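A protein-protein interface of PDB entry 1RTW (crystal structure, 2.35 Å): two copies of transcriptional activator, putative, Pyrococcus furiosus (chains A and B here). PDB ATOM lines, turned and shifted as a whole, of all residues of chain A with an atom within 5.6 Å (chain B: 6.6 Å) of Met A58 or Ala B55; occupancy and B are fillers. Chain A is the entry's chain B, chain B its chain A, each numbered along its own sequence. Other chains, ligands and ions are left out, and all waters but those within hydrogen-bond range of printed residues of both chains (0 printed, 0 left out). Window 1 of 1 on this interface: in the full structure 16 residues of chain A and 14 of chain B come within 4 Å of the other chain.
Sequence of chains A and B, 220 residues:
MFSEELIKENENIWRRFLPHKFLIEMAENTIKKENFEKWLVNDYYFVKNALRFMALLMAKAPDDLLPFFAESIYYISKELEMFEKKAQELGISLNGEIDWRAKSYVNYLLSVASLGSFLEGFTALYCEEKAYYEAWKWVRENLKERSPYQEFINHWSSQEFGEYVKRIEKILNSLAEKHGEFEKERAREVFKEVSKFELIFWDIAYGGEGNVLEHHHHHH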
ATOM      1  N   ARG A  52     -15.491 -22.543 -29.059  1.00  0.00           N
ATOM      2  CA  ARG A  52     -16.933 -22.649 -29.263  1.00  0.00           C
ATOM      3  C   ARG A  52     -17.638 -22.637 -27.907  1.00  0.00           C
ATOM      4  O   ARG A  52     -18.709 -22.057 -27.757  1.00  0.00           O
ATOM      5  CB  ARG A  52     -17.267 -23.959 -29.992  1.00  0.00           C
ATOM      6  CG  ARG A  52     -16.797 -24.020 -31.425  1.00  0.00           C
ATOM      7  CD  ARG A  52     -17.450 -25.159 -32.184  1.00  0.00           C
ATOM      8  NE  ARG A  52     -17.160 -25.085 -33.615  1.00  0.00           N
ATOM      9  CZ  ARG A  52     -16.182 -25.761 -34.209  1.00  0.00           C
ATOM     10  NH1 ARG A  52     -15.410 -26.562 -33.489  1.00  0.00           N
ATOM     11  NH2 ARG A  52     -15.964 -25.642 -35.516  1.00  0.00           N
ATOM     12  N   PHE A  53     -17.025 -23.295 -26.930  1.00  0.00           N
ATOM     13  CA  PHE A  53     -17.552 -23.381 -25.568  1.00  0.00           C
ATOM     14  C   PHE A  53     -17.634 -21.982 -24.951  1.00  0.00           C
ATOM     15  O   PHE A  53     -18.615 -21.630 -24.301  1.00  0.00           O
ATOM     16  CB  PHE A  53     -16.633 -24.284 -24.741  1.00  0.00           C
ATOM     17  CG  PHE A  53     -16.755 -24.099 -23.262  1.00  0.00           C
ATOM     18  CD1 PHE A  53     -17.805 -24.688 -22.560  1.00  0.00           C
ATOM     19  CD2 PHE A  53     -15.790 -23.384 -22.556  1.00  0.00           C
ATOM     20  CE1 PHE A  53     -17.895 -24.577 -21.183  1.00  0.00           C
ATOM     21  CE2 PHE A  53     -15.871 -23.266 -21.169  1.00  0.00           C
ATOM     22  CZ  PHE A  53     -16.933 -23.869 -20.479  1.00  0.00           C
ATOM     23  N   MET A  54     -16.580 -21.200 -25.157  1.00  0.00           N
ATOM     24  CA  MET A  54     -16.509 -19.839 -24.658  1.00  0.00           C
ATOM     25  C   MET A  54     -17.508 -18.934 -25.364  1.00  0.00           C
ATOM     26  O   MET A  54     -18.021 -17.986 -24.775  1.00  0.00           O
ATOM     27  CB  MET A  54     -15.101 -19.280 -24.863  1.00  0.00           C
ATOM     28  CG  MET A  54     -14.019 -19.969 -24.069  1.00  0.00           C
ATOM     29  SD  MET A  54     -12.277 -19.388 -24.648  1.00  0.00           S
ATOM     30  CE  MET A  54     -12.298 -17.652 -23.800  1.00  0.00           C
ATOM     31  N   ALA A  55     -17.764 -19.209 -26.638  1.00  0.00           N
ATOM     32  CA  ALA A  55     -18.695 -18.406 -27.405  1.00  0.00           C
ATOM     33  C   ALA A  55     -20.122 -18.687 -26.902  1.00  0.00           C
ATOM     34  O   ALA A  55     -20.962 -17.804 -26.832  1.00  0.00           O
ATOM     35  CB  ALA A  55     -18.540 -18.716 -28.883  1.00  0.00           C
ATOM     36  N   LEU A  56     -20.382 -19.927 -26.519  1.00  0.00           N
ATOM     37  CA  LEU A  56     -21.681 -20.285 -25.988  1.00  0.00           C
ATOM     38  C   LEU A  56     -21.907 -19.552 -24.669  1.00  0.00           C
ATOM     39  O   LEU A  56     -23.003 -19.053 -24.416  1.00  0.00           O
ATOM     40  CB  LEU A  56     -21.756 -21.782 -25.794  1.00  0.00           C
ATOM     41  CG  LEU A  56     -21.992 -22.493 -27.119  1.00  0.00           C
ATOM     42  CD1 LEU A  56     -21.907 -23.984 -26.915  1.00  0.00           C
ATOM     43  CD2 LEU A  56     -23.350 -22.116 -27.665  1.00  0.00           C
ATOM     44  N   LEU A  57     -20.856 -19.453 -23.853  1.00  0.00           N
ATOM     45  CA  LEU A  57     -20.937 -18.758 -22.580  1.00  0.00           C
ATOM     46  C   LEU A  57     -21.158 -17.268 -22.833  1.00  0.00           C
ATOM     47  O   LEU A  57     -21.990 -16.640 -22.181  1.00  0.00           O
ATOM     48  CB  LEU A  57     -19.655 -18.953 -21.769  1.00  0.00           C
ATOM     49  CG  LEU A  57     -19.422 -20.329 -21.163  1.00  0.00           C
ATOM     50  CD1 LEU A  57     -18.078 -20.357 -20.441  1.00  0.00           C
ATOM     51  CD2 LEU A  57     -20.552 -20.673 -20.205  1.00  0.00           C
ATOM     52  N   MET A  58     -20.448 -16.727 -23.824  1.00  0.00           N
ATOM     53  CA  MET A  58     -20.569 -15.311 -24.169  1.00  0.00           C
ATOM     54  C   MET A  58     -22.014 -14.908 -24.450  1.00  0.00           C
ATOM     55  O   MET A  58     -22.500 -13.896 -23.945  1.00  0.00           O
ATOM     56  CB  MET A  58     -19.682 -14.955 -25.373  1.00  0.00           C
ATOM     57  CG  MET A  58     -19.879 -13.532 -25.867  1.00  0.00           C
ATOM     58  SD  MET A  58     -18.501 -12.928 -27.119  1.00  0.00           S
ATOM     59  CE  MET A  58     -18.820 -11.022 -26.984  1.00  0.00           C
ATOM     60  N   ALA A  59     -22.704 -15.726 -25.231  1.00  0.00           N
ATOM     61  CA  ALA A  59     -24.086 -15.461 -25.587  1.00  0.00           C
ATOM     62  C   ALA A  59     -25.034 -15.357 -24.386  1.00  0.00           C
ATOM     63  O   ALA A  59     -26.042 -14.658 -24.450  1.00  0.00           O
ATOM     64  CB  ALA A  59     -24.566 -16.529 -26.535  1.00  0.00           C
ATOM     65  N   LYS A  60     -24.702 -16.067 -23.310  1.00  0.00           N
ATOM     66  CA  LYS A  60     -25.490 -16.111 -22.085  1.00  0.00           C
ATOM     67  C   LYS A  60     -24.949 -15.180 -21.010  1.00  0.00           C
ATOM     68  O   LYS A  60     -25.540 -15.083 -19.939  1.00  0.00           O
ATOM     69  CB  LYS A  60     -25.432 -17.514 -21.483  1.00  0.00           C
ATOM     70  CG  LYS A  60     -26.379 -18.539 -22.013  1.00  0.00           C
ATOM     71  CD  LYS A  60     -26.272 -19.791 -21.131  1.00  0.00           C
ATOM     72  CE  LYS A  60     -27.164 -20.919 -21.617  1.00  0.00           C
ATOM     73  NZ  LYS A  60     -26.895 -22.171 -20.851  1.00  0.00           N
ATOM     74  N   ALA A  61     -23.812 -14.540 -21.265  1.00  0.00           N
ATOM     75  CA  ALA A  61     -23.190 -13.676 -20.260  1.00  0.00           C
ATOM     76  C   ALA A  61     -23.830 -12.315 -20.023  1.00  0.00           C
ATOM     77  O   ALA A  61     -24.466 -11.747 -20.911  1.00  0.00           O
ATOM     78  CB  ALA A  61     -21.695 -13.492 -20.568  1.00  0.00           C
ATOM     79  N   LEU A  66     -19.366  -8.853 -21.623  1.00  0.00           N
ATOM     80  CA  LEU A  66     -19.208  -8.936 -23.069  1.00  0.00           C
ATOM     81  C   LEU A  66     -17.802  -8.568 -23.540  1.00  0.00           C
ATOM     82  O   LEU A  66     -17.225  -9.288 -24.349  1.00  0.00           O
ATOM     83  CB  LEU A  66     -20.277  -8.113 -23.791  1.00  0.00           C
ATOM     84  CG  LEU A  66     -21.690  -8.656 -23.543  1.00  0.00           C
ATOM     85  CD1 LEU A  66     -22.728  -7.815 -24.265  1.00  0.00           C
ATOM     86  CD2 LEU A  66     -21.781 -10.100 -23.998  1.00  0.00           C
ATOM     87  N   PRO A  67     -17.223  -7.464 -23.019  1.00  0.00           N
ATOM     88  CA  PRO A  67     -15.868  -7.059 -23.426  1.00  0.00           C
ATOM     89  C   PRO A  67     -14.827  -8.125 -23.047  1.00  0.00           C
ATOM     90  O   PRO A  67     -13.913  -8.414 -23.820  1.00  0.00           O
ATOM     91  CB  PRO A  67     -15.643  -5.763 -22.629  1.00  0.00           C
ATOM     92  CG  PRO A  67     -17.022  -5.212 -22.472  1.00  0.00           C
ATOM     93  CD  PRO A  67     -17.807  -6.453 -22.113  1.00  0.00           C
ATOM     94  N   PHE A  69     -15.291 -11.393 -22.652  1.00  0.00           N
ATOM     95  CA  PHE A  69     -15.440 -12.531 -23.543  1.00  0.00           C
ATOM     96  C   PHE A  69     -14.923 -12.240 -24.934  1.00  0.00           C
ATOM     97  O   PHE A  69     -14.334 -13.115 -25.564  1.00  0.00           O
ATOM     98  CB  PHE A  69     -16.891 -13.002 -23.589  1.00  0.00           C
ATOM     99  CG  PHE A  69     -17.234 -14.009 -22.516  1.00  0.00           C
ATOM    100  CD1 PHE A  69     -16.813 -15.329 -22.629  1.00  0.00           C
ATOM    101  CD2 PHE A  69     -17.981 -13.644 -21.409  1.00  0.00           C
ATOM    102  CE1 PHE A  69     -17.138 -16.274 -21.656  1.00  0.00           C
ATOM    103  CE2 PHE A  69     -18.309 -14.582 -20.428  1.00  0.00           C
ATOM    104  CZ  PHE A  69     -17.890 -15.899 -20.552  1.00  0.00           C
ATOM    105  N   ALA A  70     -15.119 -11.010 -25.410  1.00  0.00           N
ATOM    106  CA  ALA A  70     -14.633 -10.637 -26.740  1.00  0.00           C
ATOM    107  C   ALA A  70     -13.111 -10.703 -26.807  1.00  0.00           C
ATOM    108  O   ALA A  70     -12.548 -11.265 -27.753  1.00  0.00           O
ATOM    109  CB  ALA A  70     -15.108  -9.259 -27.115  1.00  0.00           C
ATOM    110  N   ILE A  73     -11.800 -14.564 -26.086  1.00  0.00           N
ATOM    111  CA  ILE A  73     -11.948 -15.430 -27.259  1.00  0.00           C
ATOM    112  C   ILE A  73     -10.897 -15.084 -28.310  1.00  0.00           C
ATOM    113  O   ILE A  73     -10.273 -15.981 -28.894  1.00  0.00           O
ATOM    114  CB  ILE A  73     -13.352 -15.335 -27.851  1.00  0.00           C
ATOM    115  CG1 ILE A  73     -14.347 -15.978 -26.883  1.00  0.00           C
ATOM    116  CG2 ILE A  73     -13.413 -16.012 -29.219  1.00  0.00           C
ATOM    117  CD1 ILE A  73     -15.797 -15.884 -27.346  1.00  0.00           C
ATOM    118  N   PHE A 118     -25.210 -20.375 -16.251  1.00  0.00           N
ATOM    119  CA  PHE A 118     -24.020 -19.609 -16.617  1.00  0.00           C
ATOM    120  C   PHE A 118     -22.885 -19.900 -15.630  1.00  0.00           C
ATOM    121  O   PHE A 118     -21.727 -20.068 -16.031  1.00  0.00           O
ATOM    122  CB  PHE A 118     -24.319 -18.106 -16.648  1.00  0.00           C
ATOM    123  CG  PHE A 118     -23.149 -17.267 -17.083  1.00  0.00           C
ATOM    124  CD1 PHE A 118     -22.635 -17.384 -18.368  1.00  0.00           C
ATOM    125  CD2 PHE A 118     -22.552 -16.363 -16.210  1.00  0.00           C
ATOM    126  CE1 PHE A 118     -21.559 -16.628 -18.774  1.00  0.00           C
ATOM    127  CE2 PHE A 118     -21.468 -15.596 -16.612  1.00  0.00           C
ATOM    128  CZ  PHE A 118     -20.972 -15.731 -17.895  1.00  0.00           C
ATOM    129  N   LYS B  48     -24.844  -4.741 -28.537  1.00  0.00           N
ATOM    130  CA  LYS B  48     -24.479  -5.673 -27.480  1.00  0.00           C
ATOM    131  C   LYS B  48     -25.007  -7.058 -27.812  1.00  0.00           C
ATOM    132  O   LYS B  48     -24.300  -8.059 -27.719  1.00  0.00           O
ATOM    133  CB  LYS B  48     -25.043  -5.218 -26.136  1.00  0.00           C
ATOM    134  CG  LYS B  48     -24.234  -4.103 -25.491  1.00  0.00           C
ATOM    135  CD  LYS B  48     -24.817  -3.700 -24.145  1.00  0.00           C
ATOM    136  CE  LYS B  48     -26.215  -3.129 -24.314  1.00  0.00           C
ATOM    137  NZ  LYS B  48     -26.821  -2.759 -23.015  1.00  0.00           N
ATOM    138  N   ALA B  50     -26.011  -8.107 -30.829  1.00  0.00           N
ATOM    139  CA  ALA B  50     -25.482  -8.584 -32.100  1.00  0.00           C
ATOM    140  C   ALA B  50     -24.221  -9.406 -31.783  1.00  0.00           C
ATOM    141  O   ALA B  50     -23.914 -10.394 -32.454  1.00  0.00           O
ATOM    142  CB  ALA B  50     -25.135  -7.409 -32.991  1.00  0.00           C
ATOM    143  N   LEU B  51     -23.541  -9.017 -30.709  1.00  0.00           N
ATOM    144  CA  LEU B  51     -22.338  -9.689 -30.248  1.00  0.00           C
ATOM    145  C   LEU B  51     -22.667 -11.096 -29.723  1.00  0.00           C
ATOM    146  O   LEU B  51     -21.883 -12.035 -29.896  1.00  0.00           O
ATOM    147  CB  LEU B  51     -21.671  -8.847 -29.156  1.00  0.00           C
ATOM    148  CG  LEU B  51     -20.354  -8.103 -29.432  1.00  0.00           C
ATOM    149  CD1 LEU B  51     -20.249  -7.679 -30.884  1.00  0.00           C
ATOM    150  CD2 LEU B  51     -20.205  -6.886 -28.467  1.00  0.00           C
ATOM    151  N   ARG B  52     -23.817 -11.236 -29.066  1.00  0.00           N
ATOM    152  CA  ARG B  52     -24.234 -12.532 -28.544  1.00  0.00           C
ATOM    153  C   ARG B  52     -24.676 -13.382 -29.723  1.00  0.00           C
ATOM    154  O   ARG B  52     -24.456 -14.592 -29.749  1.00  0.00           O
ATOM    155  CB  ARG B  52     -25.375 -12.388 -27.537  1.00  0.00           C
ATOM    156  CG  ARG B  52     -24.987 -11.687 -26.246  1.00  0.00           C
ATOM    157  CD  ARG B  52     -26.155 -11.688 -25.283  1.00  0.00           C
ATOM    158  NE  ARG B  52     -25.772 -11.178 -23.974  1.00  0.00           N
ATOM    159  CZ  ARG B  52     -26.035  -9.949 -23.552  1.00  0.00           C
ATOM    160  NH1 ARG B  52     -26.702  -9.102 -24.332  1.00  0.00           N
ATOM    161  NH2 ARG B  52     -25.550  -9.534 -22.391  1.00  0.00           N
ATOM    162  N   PHE B  53     -25.283 -12.720 -30.701  1.00  0.00           N
ATOM    163  CA  PHE B  53     -25.745 -13.345 -31.932  1.00  0.00           C
ATOM    164  C   PHE B  53     -24.536 -13.940 -32.685  1.00  0.00           C
ATOM    165  O   PHE B  53     -24.572 -15.075 -33.162  1.00  0.00           O
ATOM    166  CB  PHE B  53     -26.434 -12.265 -32.793  1.00  0.00           C
ATOM    167  CG  PHE B  53     -26.658 -12.666 -34.221  1.00  0.00           C
ATOM    168  CD1 PHE B  53     -27.552 -13.672 -34.541  1.00  0.00           C
ATOM    169  CD2 PHE B  53     -25.967 -12.035 -35.242  1.00  0.00           C
ATOM    170  CE1 PHE B  53     -27.757 -14.050 -35.863  1.00  0.00           C
ATOM    171  CE2 PHE B  53     -26.164 -12.404 -36.569  1.00  0.00           C
ATOM    172  CZ  PHE B  53     -27.059 -13.414 -36.878  1.00  0.00           C
ATOM    173  N   MET B  54     -23.468 -13.158 -32.771  1.00  0.00           N
ATOM    174  CA  MET B  54     -22.255 -13.584 -33.451  1.00  0.00           C
ATOM    175  C   MET B  54     -21.564 -14.728 -32.728  1.00  0.00           C
ATOM    176  O   MET B  54     -20.992 -15.610 -33.366  1.00  0.00           O
ATOM    177  CB  MET B  54     -21.300 -12.407 -33.602  1.00  0.00           C
ATOM    178  CG  MET B  54     -21.752 -11.387 -34.614  1.00  0.00           C
ATOM    179  SD  MET B  54     -20.654  -9.804 -34.498  1.00  0.00           S
ATOM    180  CE  MET B  54     -19.134 -10.425 -35.508  1.00  0.00           C
ATOM    181  N   ALA B  55     -21.597 -14.701 -31.400  1.00  0.00           N
ATOM    182  CA  ALA B  55     -20.981 -15.762 -30.602  1.00  0.00           C
ATOM    183  C   ALA B  55     -21.749 -17.059 -30.789  1.00  0.00           C
ATOM    184  O   ALA B  55     -21.158 -18.131 -30.857  1.00  0.00           O
ATOM    185  CB  ALA B  55     -20.930 -15.381 -29.124  1.00  0.00           C
ATOM    186  N   LEU B  56     -23.067 -16.967 -30.878  1.00  0.00           N
ATOM    187  CA  LEU B  56     -23.884 -18.159 -31.083  1.00  0.00           C
ATOM    188  C   LEU B  56     -23.549 -18.788 -32.430  1.00  0.00           C
ATOM    189  O   LEU B  56     -23.514 -20.010 -32.560  1.00  0.00           O
ATOM    190  CB  LEU B  56     -25.374 -17.823 -31.025  1.00  0.00           C
ATOM    191  CG  LEU B  56     -25.983 -17.706 -29.625  1.00  0.00           C
ATOM    192  CD1 LEU B  56     -27.427 -17.245 -29.730  1.00  0.00           C
ATOM    193  CD2 LEU B  56     -25.918 -19.054 -28.918  1.00  0.00           C
ATOM    194  N   LEU B  57     -23.312 -17.945 -33.431  1.00  0.00           N
ATOM    195  CA  LEU B  57     -22.962 -18.432 -34.757  1.00  0.00           C
ATOM    196  C   LEU B  57     -21.590 -19.096 -34.706  1.00  0.00           C
ATOM    197  O   LEU B  57     -21.373 -20.133 -35.325  1.00  0.00           O
ATOM    198  CB  LEU B  57     -22.944 -17.282 -35.760  1.00  0.00           C
ATOM    199  CG  LEU B  57     -24.290 -16.658 -36.105  1.00  0.00           C
ATOM    200  CD1 LEU B  57     -24.074 -15.569 -37.151  1.00  0.00           C
ATOM    201  CD2 LEU B  57     -25.240 -17.735 -36.632  1.00  0.00           C
ATOM    202  N   MET B  58     -20.673 -18.492 -33.957  1.00  0.00           N
ATOM    203  CA  MET B  58     -19.322 -19.027 -33.828  1.00  0.00           C
ATOM    204  C   MET B  58     -19.334 -20.448 -33.267  1.00  0.00           C
ATOM    205  O   MET B  58     -18.578 -21.313 -33.710  1.00  0.00           O
ATOM    206  CB  MET B  58     -18.475 -18.121 -32.939  1.00  0.00           C
ATOM    207  CG  MET B  58     -17.126 -18.706 -32.607  1.00  0.00           C
ATOM    208  SD  MET B  58     -15.989 -17.477 -31.692  1.00  0.00           S
ATOM    209  CE  MET B  58     -14.297 -18.359 -32.003  1.00  0.00           C
ATOM    210  N   ALA B  59     -20.220 -20.675 -32.298  1.00  0.00           N
ATOM    211  CA  ALA B  59     -20.358 -21.970 -31.660  1.00  0.00           C
ATOM    212  C   ALA B  59     -20.743 -23.054 -32.662  1.00  0.00           C
ATOM    213  O   ALA B  59     -20.365 -24.214 -32.494  1.00  0.00           O
ATOM    214  CB  ALA B  59     -21.384 -21.892 -30.553  1.00  0.00           C
ATOM    215  N   LYS B  60     -21.464 -22.669 -33.711  1.00  0.00           N
ATOM    216  CA  LYS B  60     -21.912 -23.613 -34.736  1.00  0.00           C
ATOM    217  C   LYS B  60     -21.067 -23.571 -36.013  1.00  0.00           C
ATOM    218  O   LYS B  60     -21.272 -24.364 -36.927  1.00  0.00           O
ATOM    219  CB  LYS B  60     -23.362 -23.312 -35.121  1.00  0.00           C
ATOM    220  CG  LYS B  60     -24.365 -23.501 -34.013  1.00  0.00           C
ATOM    221  CD  LYS B  60     -25.761 -23.285 -34.539  1.00  0.00           C
ATOM    222  CE  LYS B  60     -26.822 -23.623 -33.504  1.00  0.00           C
ATOM    223  NZ  LYS B  60     -28.185 -23.610 -34.135  1.00  0.00           N
ATOM    224  N   PHE B  69     -14.492 -15.512 -36.942  1.00  0.00           N
ATOM    225  CA  PHE B  69     -15.406 -15.134 -35.862  1.00  0.00           C
ATOM    226  C   PHE B  69     -14.693 -14.486 -34.668  1.00  0.00           C
ATOM    227  O   PHE B  69     -15.166 -13.495 -34.130  1.00  0.00           O
ATOM    228  CB  PHE B  69     -16.234 -16.337 -35.382  1.00  0.00           C
ATOM    229  CG  PHE B  69     -17.497 -16.555 -36.171  1.00  0.00           C
ATOM    230  CD1 PHE B  69     -18.603 -15.736 -35.967  1.00  0.00           C
ATOM    231  CD2 PHE B  69     -17.570 -17.551 -37.147  1.00  0.00           C
ATOM    232  CE1 PHE B  69     -19.770 -15.896 -36.724  1.00  0.00           C
ATOM    233  CE2 PHE B  69     -18.736 -17.718 -37.911  1.00  0.00           C
ATOM    234  CZ  PHE B  69     -19.837 -16.883 -37.693  1.00  0.00           C
ATOM    235  N   ILE B  73     -15.734 -10.728 -33.864  1.00  0.00           N
ATOM    236  CA  ILE B  73     -16.360 -10.404 -32.580  1.00  0.00           C
ATOM    237  C   ILE B  73     -15.504  -9.356 -31.856  1.00  0.00           C
ATOM    238  O   ILE B  73     -16.029  -8.410 -31.269  1.00  0.00           O
ATOM    239  CB  ILE B  73     -16.575 -11.678 -31.710  1.00  0.00           C
ATOM    240  CG1 ILE B  73     -17.607 -12.584 -32.391  1.00  0.00           C
ATOM    241  CG2 ILE B  73     -17.060 -11.306 -30.325  1.00  0.00           C
ATOM    242  CD1 ILE B  73     -17.924 -13.855 -31.617  1.00  0.00           C
ATOM    243  N   SER B  77     -16.807  -5.674 -31.258  1.00  0.00           N
ATOM    244  CA  SER B  77     -16.885  -5.286 -29.843  1.00  0.00           C
ATOM    245  C   SER B  77     -16.356  -3.873 -29.600  1.00  0.00           C
ATOM    246  O   SER B  77     -16.746  -3.218 -28.637  1.00  0.00           O
ATOM    247  CB  SER B  77     -16.151  -6.279 -28.938  1.00  0.00           C
ATOM    248  OG  SER B  77     -14.742  -6.129 -29.020  1.00  0.00           O
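The backbone carbonyl oxygen (O) of Ala A61 lies within hydrogen-bond range of the guanidinium group (NH2) of Arg B52 (2.9 Å).
O of Ile B73 lies close to OG of Ser B77 (3.5 Å).
Met B58 touches Arg A52. Arg A52 touches Ala B59 (CD to O, 3.1 Å). Ala A55 touches Ala B55 (CB to O, 3.3 Å). Met B58 touches Ala A55. CB of Ala B55 touches CG of Met A58 (3.9 Å). Ala A59 touches Leu B56. CD1 of Leu A66 touches O of Lys B48, 3.8 Å away. NH2 of Arg B52 touches CD1 of Leu A66, at 3.8 Å. Ala A70 touches Ser B77. CG2 of Ile A73 touches CE of Met B58, 3.7 Å away.
Printed residues of chain B within 4 Å of Met A58: Ala B55 (3.9 Å) and Ile B73 (3.8 Å). Of chain A, only Ala A55 (3.3 Å) and Met A58 (3.9 Å) come within 4 Å of Ala B55. Printed residues of chain A within 4 Å of Leu B56: Ala A59. Of the printed residues of chain A, Lys B48 touches Leu A66. Of the printed residues of chain B, Ile A73 touches Met B58 (3.7 Å). The nearest residue of chain B that does not touch Met A58 is Arg B52 (4.04 Å). The nearest residue of chain A that does not touch Ala B55 is Ala A59 (4.3 Å).
Of the 16 printed residues of chain A, 9 touch a printed residue of chain B. Hydrophobic or aromatic side chains of chain A that line the printed part of chain B: Ala A55, Leu A56, Met A58, Ala A59, Leu A66, Ala A70 and Ile A73. Hydrophobic or aromatic side chains of chain B that line the printed part of chain A: Ala B55, Leu B56, Met B58, Ala B59 and Ile B73. Along chain B the printed residues that touch a printed residue of chain A span positions 48 to 77.
Arg A52 touches Met B58, but with the chains exchanged Met A58 does not touch Arg B52 (4.04 Å). Ala B55 touches its own counterpart, Ala A55. Ala A55 touches Met B58, and with the chains exchanged Met A58 touches Ala B55. Met A58 touches Ile B73, and with the chains exchanged Ile A73 touches Met B58. Positions printed for both chains: 52, 53, 54, 55, 56, 57, 58, 59, 60, 69 and 73.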
